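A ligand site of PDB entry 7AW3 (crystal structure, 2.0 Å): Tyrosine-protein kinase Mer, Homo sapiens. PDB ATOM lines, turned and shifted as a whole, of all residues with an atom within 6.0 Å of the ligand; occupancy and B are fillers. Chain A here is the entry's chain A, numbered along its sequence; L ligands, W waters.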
ATOM      1  N   LEU A  27      27.794  23.599 -13.981  1.00  0.00           N
ATOM      2  CA  LEU A  27      27.210  22.740 -15.022  1.00  0.00           C
ATOM      3  C   LEU A  27      28.096  21.485 -15.241  1.00  0.00           C
ATOM      4  O   LEU A  27      27.577  20.430 -15.583  1.00  0.00           O
ATOM      5  CB  LEU A  27      27.093  23.499 -16.358  1.00  0.00           C
ATOM      6  CG  LEU A  27      26.136  24.693 -16.442  1.00  0.00           C
ATOM      7  CD1 LEU A  27      26.418  25.503 -17.694  1.00  0.00           C
ATOM      8  CD2 LEU A  27      24.690  24.231 -16.472  1.00  0.00           C
ATOM      9  N   GLY A  28      29.403  21.652 -15.083  1.00  0.00           N
ATOM     10  CA  GLY A  28      30.419  20.634 -15.301  1.00  0.00           C
ATOM     11  C   GLY A  28      31.729  21.021 -14.636  1.00  0.00           C
ATOM     12  O   GLY A  28      31.999  22.207 -14.451  1.00  0.00           O
ATOM     13  N   GLU A  29      32.520  20.027 -14.256  1.00  0.00           N
ATOM     14  CA  GLU A  29      33.772  20.281 -13.540  1.00  0.00           C
ATOM     15  C   GLU A  29      34.814  19.254 -13.905  1.00  0.00           C
ATOM     16  O   GLU A  29      34.631  18.075 -13.638  1.00  0.00           O
ATOM     17  CB  GLU A  29      33.486  20.241 -12.026  1.00  0.00           C
ATOM     18  CG  GLU A  29      34.494  20.981 -11.176  1.00  0.00           C
ATOM     19  CD  GLU A  29      34.088  21.138  -9.723  1.00  0.00           C
ATOM     20  OE1 GLU A  29      33.273  20.318  -9.229  1.00  0.00           O
ATOM     21  OE2 GLU A  29      34.578  22.089  -9.076  1.00  0.00           O
ATOM     22  N   VAL A  35      32.664  24.723 -15.671  1.00  0.00           N
ATOM     23  CA  VAL A  35      31.702  25.444 -16.490  1.00  0.00           C
ATOM     24  C   VAL A  35      30.521  25.719 -15.559  1.00  0.00           C
ATOM     25  O   VAL A  35      30.052  24.805 -14.880  1.00  0.00           O
ATOM     26  CB  VAL A  35      31.285  24.739 -17.813  1.00  0.00           C
ATOM     27  CG1 VAL A  35      30.348  25.625 -18.636  1.00  0.00           C
ATOM     28  CG2 VAL A  35      32.495  24.322 -18.632  1.00  0.00           C
ATOM     29  N   MET A  36      30.114  26.983 -15.461  1.00  0.00           N
ATOM     30  CA  MET A  36      29.015  27.420 -14.607  1.00  0.00           C
ATOM     31  C   MET A  36      28.001  28.180 -15.454  1.00  0.00           C
ATOM     32  O   MET A  36      28.378  28.789 -16.462  1.00  0.00           O
ATOM     33  CB  MET A  36      29.514  28.388 -13.512  1.00  0.00           C
ATOM     34  CG  MET A  36      30.508  27.784 -12.541  1.00  0.00           C
ATOM     35  SD  MET A  36      31.089  29.065 -11.372  1.00  0.00           S
ATOM     36  CE  MET A  36      32.507  29.649 -12.246  1.00  0.00           C
ATOM     37  N   ALA A  51      27.143  30.754 -20.410  1.00  0.00           N
ATOM     38  CA  ALA A  51      27.956  29.686 -19.833  1.00  0.00           C
ATOM     39  C   ALA A  51      29.296  30.327 -19.560  1.00  0.00           C
ATOM     40  O   ALA A  51      29.759  31.120 -20.374  1.00  0.00           O
ATOM     41  CB  ALA A  51      28.108  28.507 -20.781  1.00  0.00           C
ATOM     42  N   LYS A  53      33.209  29.570 -18.453  1.00  0.00           N
ATOM     43  CA  LYS A  53      34.247  28.542 -18.294  1.00  0.00           C
ATOM     44  C   LYS A  53      35.415  29.133 -17.517  1.00  0.00           C
ATOM     45  O   LYS A  53      35.889  30.224 -17.862  1.00  0.00           O
ATOM     46  CB  LYS A  53      34.685  27.995 -19.658  1.00  0.00           C
ATOM     47  CG  LYS A  53      35.614  26.791 -19.533  1.00  0.00           C
ATOM     48  CD  LYS A  53      36.236  26.399 -20.853  1.00  0.00           C
ATOM     49  CE  LYS A  53      37.087  25.160 -20.667  1.00  0.00           C
ATOM     50  NZ  LYS A  53      37.650  24.678 -21.963  1.00  0.00           N
ATOM     51  N   ILE A  84      31.355  28.989 -32.387  1.00  0.00           N
ATOM     52  CA  ILE A  84      30.819  29.543 -31.116  1.00  0.00           C
ATOM     53  C   ILE A  84      31.335  30.979 -30.932  1.00  0.00           C
ATOM     54  O   ILE A  84      32.492  31.278 -31.274  1.00  0.00           O
ATOM     55  CB  ILE A  84      31.097  28.647 -29.875  1.00  0.00           C
ATOM     56  CG1 ILE A  84      30.149  29.042 -28.686  1.00  0.00           C
ATOM     57  CG2 ILE A  84      32.582  28.699 -29.457  1.00  0.00           C
ATOM     58  CD1 ILE A  84      29.885  27.946 -27.694  1.00  0.00           C
ATOM     59  N   LEU A 105      30.475  32.603 -22.777  1.00  0.00           N
ATOM     60  CA  LEU A 105      29.949  32.072 -24.035  1.00  0.00           C
ATOM     61  C   LEU A 105      28.443  32.049 -24.035  1.00  0.00           C
ATOM     62  O   LEU A 105      27.868  31.985 -22.958  1.00  0.00           O
ATOM     63  CB  LEU A 105      30.485  30.619 -24.188  1.00  0.00           C
ATOM     64  CG  LEU A 105      32.002  30.497 -24.153  1.00  0.00           C
ATOM     65  CD1 LEU A 105      32.436  29.138 -23.755  1.00  0.00           C
ATOM     66  CD2 LEU A 105      32.606  30.862 -25.486  1.00  0.00           C
ATOM     67  N   PRO A 106      27.740  31.984 -25.190  1.00  0.00           N
ATOM     68  CA  PRO A 106      26.268  31.866 -25.152  1.00  0.00           C
ATOM     69  C   PRO A 106      25.912  30.527 -24.510  1.00  0.00           C
ATOM     70  O   PRO A 106      26.668  29.575 -24.647  1.00  0.00           O
ATOM     71  CB  PRO A 106      25.890  31.825 -26.633  1.00  0.00           C
ATOM     72  CG  PRO A 106      27.034  32.541 -27.332  1.00  0.00           C
ATOM     73  CD  PRO A 106      28.214  32.001 -26.589  1.00  0.00           C
ATOM     74  N   PHE A 107      24.764  30.477 -23.812  1.00  0.00           N
ATOM     75  CA  PHE A 107      24.294  29.262 -23.182  1.00  0.00           C
ATOM     76  C   PHE A 107      23.517  28.461 -24.209  1.00  0.00           C
ATOM     77  O   PHE A 107      22.561  28.976 -24.800  1.00  0.00           O
ATOM     78  CB  PHE A 107      23.431  29.587 -21.963  1.00  0.00           C
ATOM     79  CG  PHE A 107      22.993  28.345 -21.231  1.00  0.00           C
ATOM     80  CD1 PHE A 107      23.817  27.745 -20.292  1.00  0.00           C
ATOM     81  CD2 PHE A 107      21.771  27.750 -21.521  1.00  0.00           C
ATOM     82  CE1 PHE A 107      23.432  26.576 -19.653  1.00  0.00           C
ATOM     83  CE2 PHE A 107      21.361  26.603 -20.857  1.00  0.00           C
ATOM     84  CZ  PHE A 107      22.210  26.011 -19.937  1.00  0.00           C
ATOM     85  N   MET A 108      23.884  27.177 -24.367  1.00  0.00           N
ATOM     86  CA  MET A 108      23.294  26.239 -25.306  1.00  0.00           C
ATOM     87  C   MET A 108      22.474  25.219 -24.540  1.00  0.00           C
ATOM     88  O   MET A 108      23.053  24.252 -24.029  1.00  0.00           O
ATOM     89  CB  MET A 108      24.407  25.512 -26.097  1.00  0.00           C
ATOM     90  CG  MET A 108      25.565  26.409 -26.541  1.00  0.00           C
ATOM     91  SD  MET A 108      25.174  27.069 -28.158  1.00  0.00           S
ATOM     92  CE  MET A 108      26.636  27.752 -28.589  1.00  0.00           C
ATOM     93  N   LYS A 109      21.139  25.410 -24.466  1.00  0.00           N
ATOM     94  CA  LYS A 109      20.242  24.504 -23.738  1.00  0.00           C
ATOM     95  C   LYS A 109      20.336  23.040 -24.234  1.00  0.00           C
ATOM     96  O   LYS A 109      20.235  22.133 -23.416  1.00  0.00           O
ATOM     97  CB  LYS A 109      18.788  24.996 -23.712  1.00  0.00           C
ATOM     98  CG  LYS A 109      18.151  25.178 -25.085  1.00  0.00           C
ATOM     99  CD  LYS A 109      16.656  25.375 -25.023  1.00  0.00           C
ATOM    100  CE  LYS A 109      16.050  25.137 -26.377  1.00  0.00           C
ATOM    101  NZ  LYS A 109      14.902  24.195 -26.313  1.00  0.00           N
ATOM    102  N   GLY A 111      23.023  21.511 -25.317  1.00  0.00           N
ATOM    103  CA  GLY A 111      24.324  20.980 -24.949  1.00  0.00           C
ATOM    104  C   GLY A 111      25.233  20.603 -26.110  1.00  0.00           C
ATOM    105  O   GLY A 111      25.126  21.169 -27.211  1.00  0.00           O
ATOM    106  N   ASP A 112      26.184  19.723 -25.840  1.00  0.00           N
ATOM    107  CA  ASP A 112      27.164  19.267 -26.833  1.00  0.00           C
ATOM    108  C   ASP A 112      26.550  18.228 -27.740  1.00  0.00           C
ATOM    109  O   ASP A 112      25.578  17.522 -27.367  1.00  0.00           O
ATOM    110  CB  ASP A 112      28.426  18.743 -26.152  1.00  0.00           C
ATOM    111  CG  ASP A 112      28.239  17.391 -25.505  1.00  0.00           C
ATOM    112  OD1 ASP A 112      27.829  17.350 -24.330  1.00  0.00           O
ATOM    113  OD2 ASP A 112      28.528  16.375 -26.152  1.00  0.00           O
ATOM    114  N   THR A 115      26.686  14.227 -26.555  1.00  0.00           N
ATOM    115  CA  THR A 115      25.644  13.884 -25.579  1.00  0.00           C
ATOM    116  C   THR A 115      24.262  13.831 -26.262  1.00  0.00           C
ATOM    117  O   THR A 115      23.519  12.886 -26.036  1.00  0.00           O
ATOM    118  CB  THR A 115      25.708  14.793 -24.369  1.00  0.00           C
ATOM    119  OG1 THR A 115      27.063  14.838 -23.932  1.00  0.00           O
ATOM    120  CG2 THR A 115      24.835  14.294 -23.210  1.00  0.00           C
ATOM    121  N   TYR A 119      21.750  10.703 -26.320  1.00  0.00           N
ATOM    122  CA  TYR A 119      20.389  10.836 -25.778  1.00  0.00           C
ATOM    123  C   TYR A 119      19.331  10.411 -26.786  1.00  0.00           C
ATOM    124  O   TYR A 119      18.277   9.890 -26.401  1.00  0.00           O
ATOM    125  CB  TYR A 119      20.103  12.300 -25.368  1.00  0.00           C
ATOM    126  CG  TYR A 119      20.706  12.799 -24.065  1.00  0.00           C
ATOM    127  CD1 TYR A 119      21.222  11.912 -23.116  1.00  0.00           C
ATOM    128  CD2 TYR A 119      20.717  14.167 -23.756  1.00  0.00           C
ATOM    129  CE1 TYR A 119      21.741  12.369 -21.907  1.00  0.00           C
ATOM    130  CE2 TYR A 119      21.208  14.626 -22.529  1.00  0.00           C
ATOM    131  CZ  TYR A 119      21.729  13.730 -21.616  1.00  0.00           C
ATOM    132  OH  TYR A 119      22.236  14.196 -20.427  1.00  0.00           O
ATOM    133  N   ARG A 161      32.237  15.887 -29.118  1.00  0.00           N
ATOM    134  CA  ARG A 161      32.022  16.437 -27.745  1.00  0.00           C
ATOM    135  C   ARG A 161      32.286  17.961 -27.681  1.00  0.00           C
ATOM    136  O   ARG A 161      31.724  18.627 -26.814  1.00  0.00           O
ATOM    137  CB  ARG A 161      32.881  15.697 -26.703  1.00  0.00           C
ATOM    138  CG  ARG A 161      34.378  15.893 -26.917  1.00  0.00           C
ATOM    139  CD  ARG A 161      35.269  15.034 -26.044  1.00  0.00           C
ATOM    140  NE  ARG A 161      36.668  15.197 -26.436  1.00  0.00           N
ATOM    141  CZ  ARG A 161      37.331  14.370 -27.245  1.00  0.00           C
ATOM    142  NH1 ARG A 161      36.723  13.295 -27.732  1.00  0.00           N
ATOM    143  NH2 ARG A 161      38.595  14.605 -27.553  1.00  0.00           N
ATOM    144  N   ASN A 162      33.139  18.475 -28.586  1.00  0.00           N
ATOM    145  CA  ASN A 162      33.532  19.886 -28.684  1.00  0.00           C
ATOM    146  C   ASN A 162      32.678  20.709 -29.676  1.00  0.00           C
ATOM    147  O   ASN A 162      33.011  21.840 -29.985  1.00  0.00           O
ATOM    148  CB  ASN A 162      35.043  19.985 -28.999  1.00  0.00           C
ATOM    149  CG  ASN A 162      35.881  19.444 -27.848  1.00  0.00           C
ATOM    150  OD1 ASN A 162      35.525  19.544 -26.674  1.00  0.00           O
ATOM    151  ND2 ASN A 162      36.962  18.801 -28.126  1.00  0.00           N
ATOM    152  N   CYS A 163      31.585  20.138 -30.157  1.00  0.00           N
ATOM    153  CA  CYS A 163      30.638  20.803 -31.042  1.00  0.00           C
ATOM    154  C   CYS A 163      29.376  21.060 -30.236  1.00  0.00           C
ATOM    155  O   CYS A 163      28.962  20.200 -29.479  1.00  0.00           O
ATOM    156  CB  CYS A 163      30.365  19.960 -32.272  1.00  0.00           C
ATOM    157  SG  CYS A 163      31.818  19.759 -33.328  1.00  0.00           S
ATOM    158  N   MET A 164      28.824  22.247 -30.323  1.00  0.00           N
ATOM    159  CA  MET A 164      27.663  22.616 -29.517  1.00  0.00           C
ATOM    160  C   MET A 164      26.449  22.746 -30.412  1.00  0.00           C
ATOM    161  O   MET A 164      26.620  23.071 -31.574  1.00  0.00           O
ATOM    162  CB  MET A 164      27.972  23.960 -28.802  1.00  0.00           C
ATOM    163  CG  MET A 164      29.016  23.825 -27.704  1.00  0.00           C
ATOM    164  SD  MET A 164      28.410  22.700 -26.411  1.00  0.00           S
ATOM    165  CE  MET A 164      29.521  22.885 -25.274  1.00  0.00           C
ATOM    166  N   ALA A 174      33.399  24.562 -31.101  1.00  0.00           N
ATOM    167  CA  ALA A 174      33.750  25.176 -29.811  1.00  0.00           C
ATOM    168  C   ALA A 174      35.046  24.573 -29.263  1.00  0.00           C
ATOM    169  O   ALA A 174      35.587  23.672 -29.890  1.00  0.00           O
ATOM    170  CB  ALA A 174      32.609  24.939 -28.828  1.00  0.00           C
ATOM    171  N   ASP A 175      35.562  25.085 -28.118  1.00  0.00           N
ATOM    172  CA  ASP A 175      36.784  24.591 -27.446  1.00  0.00           C
ATOM    173  C   ASP A 175      38.082  24.526 -28.329  1.00  0.00           C
ATOM    174  O   ASP A 175      38.790  23.504 -28.366  1.00  0.00           O
ATOM    175  CB  ASP A 175      36.498  23.221 -26.799  1.00  0.00           C
ATOM    176  CG  ASP A 175      37.415  22.942 -25.640  1.00  0.00           C
ATOM    177  OD1 ASP A 175      37.193  23.522 -24.565  1.00  0.00           O
ATOM    178  OD2 ASP A 175      38.366  22.142 -25.812  1.00  0.00           O
HETATM  179  C1  LIG L   1      28.730  18.502 -20.750  1.00  0.00           C
HETATM  180  C2  LIG L   1      29.609  19.602 -21.254  1.00  0.00           C
HETATM  181  C3  LIG L   1      29.959  20.829 -20.701  1.00  0.00           C
HETATM  182  C4  LIG L   1      34.093  22.074 -23.749  1.00  0.00           C
HETATM  183  C5  LIG L   1      32.738  22.783 -23.473  1.00  0.00           C
HETATM  184  C6  LIG L   1      32.703  23.125 -24.991  1.00  0.00           C
HETATM  185  C7  LIG L   1      32.552  23.787 -22.305  1.00  0.00           C
HETATM  186  C8  LIG L   1      31.018  25.441 -23.250  1.00  0.00           C
HETATM  187  C9  LIG L   1      29.620  25.933 -23.347  1.00  0.00           C
HETATM  188  C10 LIG L   1      29.240  27.089 -23.995  1.00  0.00           C
HETATM  189  C11 LIG L   1      27.344  26.203 -23.235  1.00  0.00           C
HETATM  190  C12 LIG L   1      28.387  25.345 -22.842  1.00  0.00           C
HETATM  191  C13 LIG L   1      28.052  24.207 -22.111  1.00  0.00           C
HETATM  192  C14 LIG L   1      29.511  21.365 -19.372  1.00  0.00           C
HETATM  193  F1  LIG L   1      30.421  21.155 -18.426  1.00  0.00           F
HETATM  194  F2  LIG L   1      28.370  20.796 -18.960  1.00  0.00           F
HETATM  195  F3  LIG L   1      29.292  22.688 -19.401  1.00  0.00           F
HETATM  196  N1  LIG L   1      30.839  21.585 -21.440  1.00  0.00           N
HETATM  197  C15 LIG L   1      31.150  20.980 -22.570  1.00  0.00           C
HETATM  198  S1  LIG L   1      30.378  19.430 -22.802  1.00  0.00           S
HETATM  199  O1  LIG L   1      28.945  18.102 -19.594  1.00  0.00           O
HETATM  200  N2  LIG L   1      27.744  18.014 -21.497  1.00  0.00           N
HETATM  201  C16 LIG L   1      26.898  16.926 -21.041  1.00  0.00           C
HETATM  202  N3  LIG L   1      31.978  21.489 -23.508  1.00  0.00           N
HETATM  203  C17 LIG L   1      33.429  21.778 -25.108  1.00  0.00           C
HETATM  204  C18 LIG L   1      32.311  20.781 -24.748  1.00  0.00           C
HETATM  205  N4  LIG L   1      31.252  24.413 -22.424  1.00  0.00           N
HETATM  206  O2  LIG L   1      31.907  25.947 -23.932  1.00  0.00           O
HETATM  207  C19 LIG L   1      26.709  24.002 -21.827  1.00  0.00           C
HETATM  208 CL1  LIG L   1      26.227  22.594 -20.916  1.00  0.00          CL
HETATM  209  C20 LIG L   1      25.741  24.935 -22.260  1.00  0.00           C
HETATM  210  N5  LIG L   1      26.046  26.042 -22.958  1.00  0.00           N
HETATM  211  N6  LIG L   1      27.882  27.253 -23.932  1.00  0.00           N
HETATM  212  O   HOH W   1      24.902  18.107 -23.195  1.00  0.00           O
HETATM  213  O   HOH W   2      34.348  26.155 -25.149  1.00  0.00           O
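The backbone NH (N) of Asp 112 sits close to the side-chain sulfur (SD) of Met 164, at 3.8 Å.
The side-chain carboxylate of Asp 112 is in hydrogen-bond range of the side-chain hydroxyl of Thr 115, at 2.7 Å.
The backbone NH (N) of Val 35 is in hydrogen-bond range of the backbone carbonyl oxygen (O) of Gly 28 (2.9 Å).
N of Leu 27 is in hydrogen-bond range of O of Val 35 (2.7 Å).
The backbone NH (N) of Leu 105 sits at hydrogen-bond distance from the backbone carbonyl oxygen (O) of Ala 51 (2.9 Å).
The backbone carbonyl oxygen (O) of Asn 162 sits at hydrogen-bond distance from the backbone NH (N) of Ala 174 (3.0 Å).
The side-chain carboxylate (OD1) of Asp 175 is in salt-bridge range of the side-chain amino group (NZ) of Lys 53 (2.9 Å).
O of Pro 106 is in hydrogen-bond range of N6 of the ligand, at 2.7 Å.
The backbone NH of Met 108 lies within hydrogen-bond range of a nitrogen (N5) of the ligand (2.8 Å).
OD1 of Asp 112 sits at hydrogen-bond distance from N2 of the ligand, 2.9 Å away.
A fluorine (F2) of the ligand sits close to the backbone carbonyl oxygen (O) of Leu 27, 3.5 Å away.
Merely in contact with the ligand: Arg 161 (3.0 Å), Gly 28 (3.2 Å), Met 164 (3.2 Å), Val 35 (3.2 Å), Leu 105 (3.2 Å), Ala 51 (3.4 Å), Asn 162 (3.4 Å), Asp 175 (3.5 Å), Thr 115 (3.6 Å), Phe 107 (3.7 Å) and Ile 84 (3.9 Å).
Hydrophobic or aromatic side chains that line the ligand: Leu 27, Val 35, Ala 51, Ile 84, Leu 105, Phe 107, Met 108 and Met 164.
15 residues have an atom within 4 Å of the ligand: Leu 27, Gly 28, Val 35, Ala 51, Ile 84, Leu 105, Pro 106, Phe 107, Met 108, Asp 112, Thr 115, Arg 161, Asn 162, Met 164 and Asp 175.
Water W2 bridges O2 of the ligand (2.7 Å) and N of Asp 175 (3.4 Å).
Water W1 lies within hydrogen-bond range of OD1 of Asp 112 (3.2 Å) and N2 of the ligand (3.3 Å).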
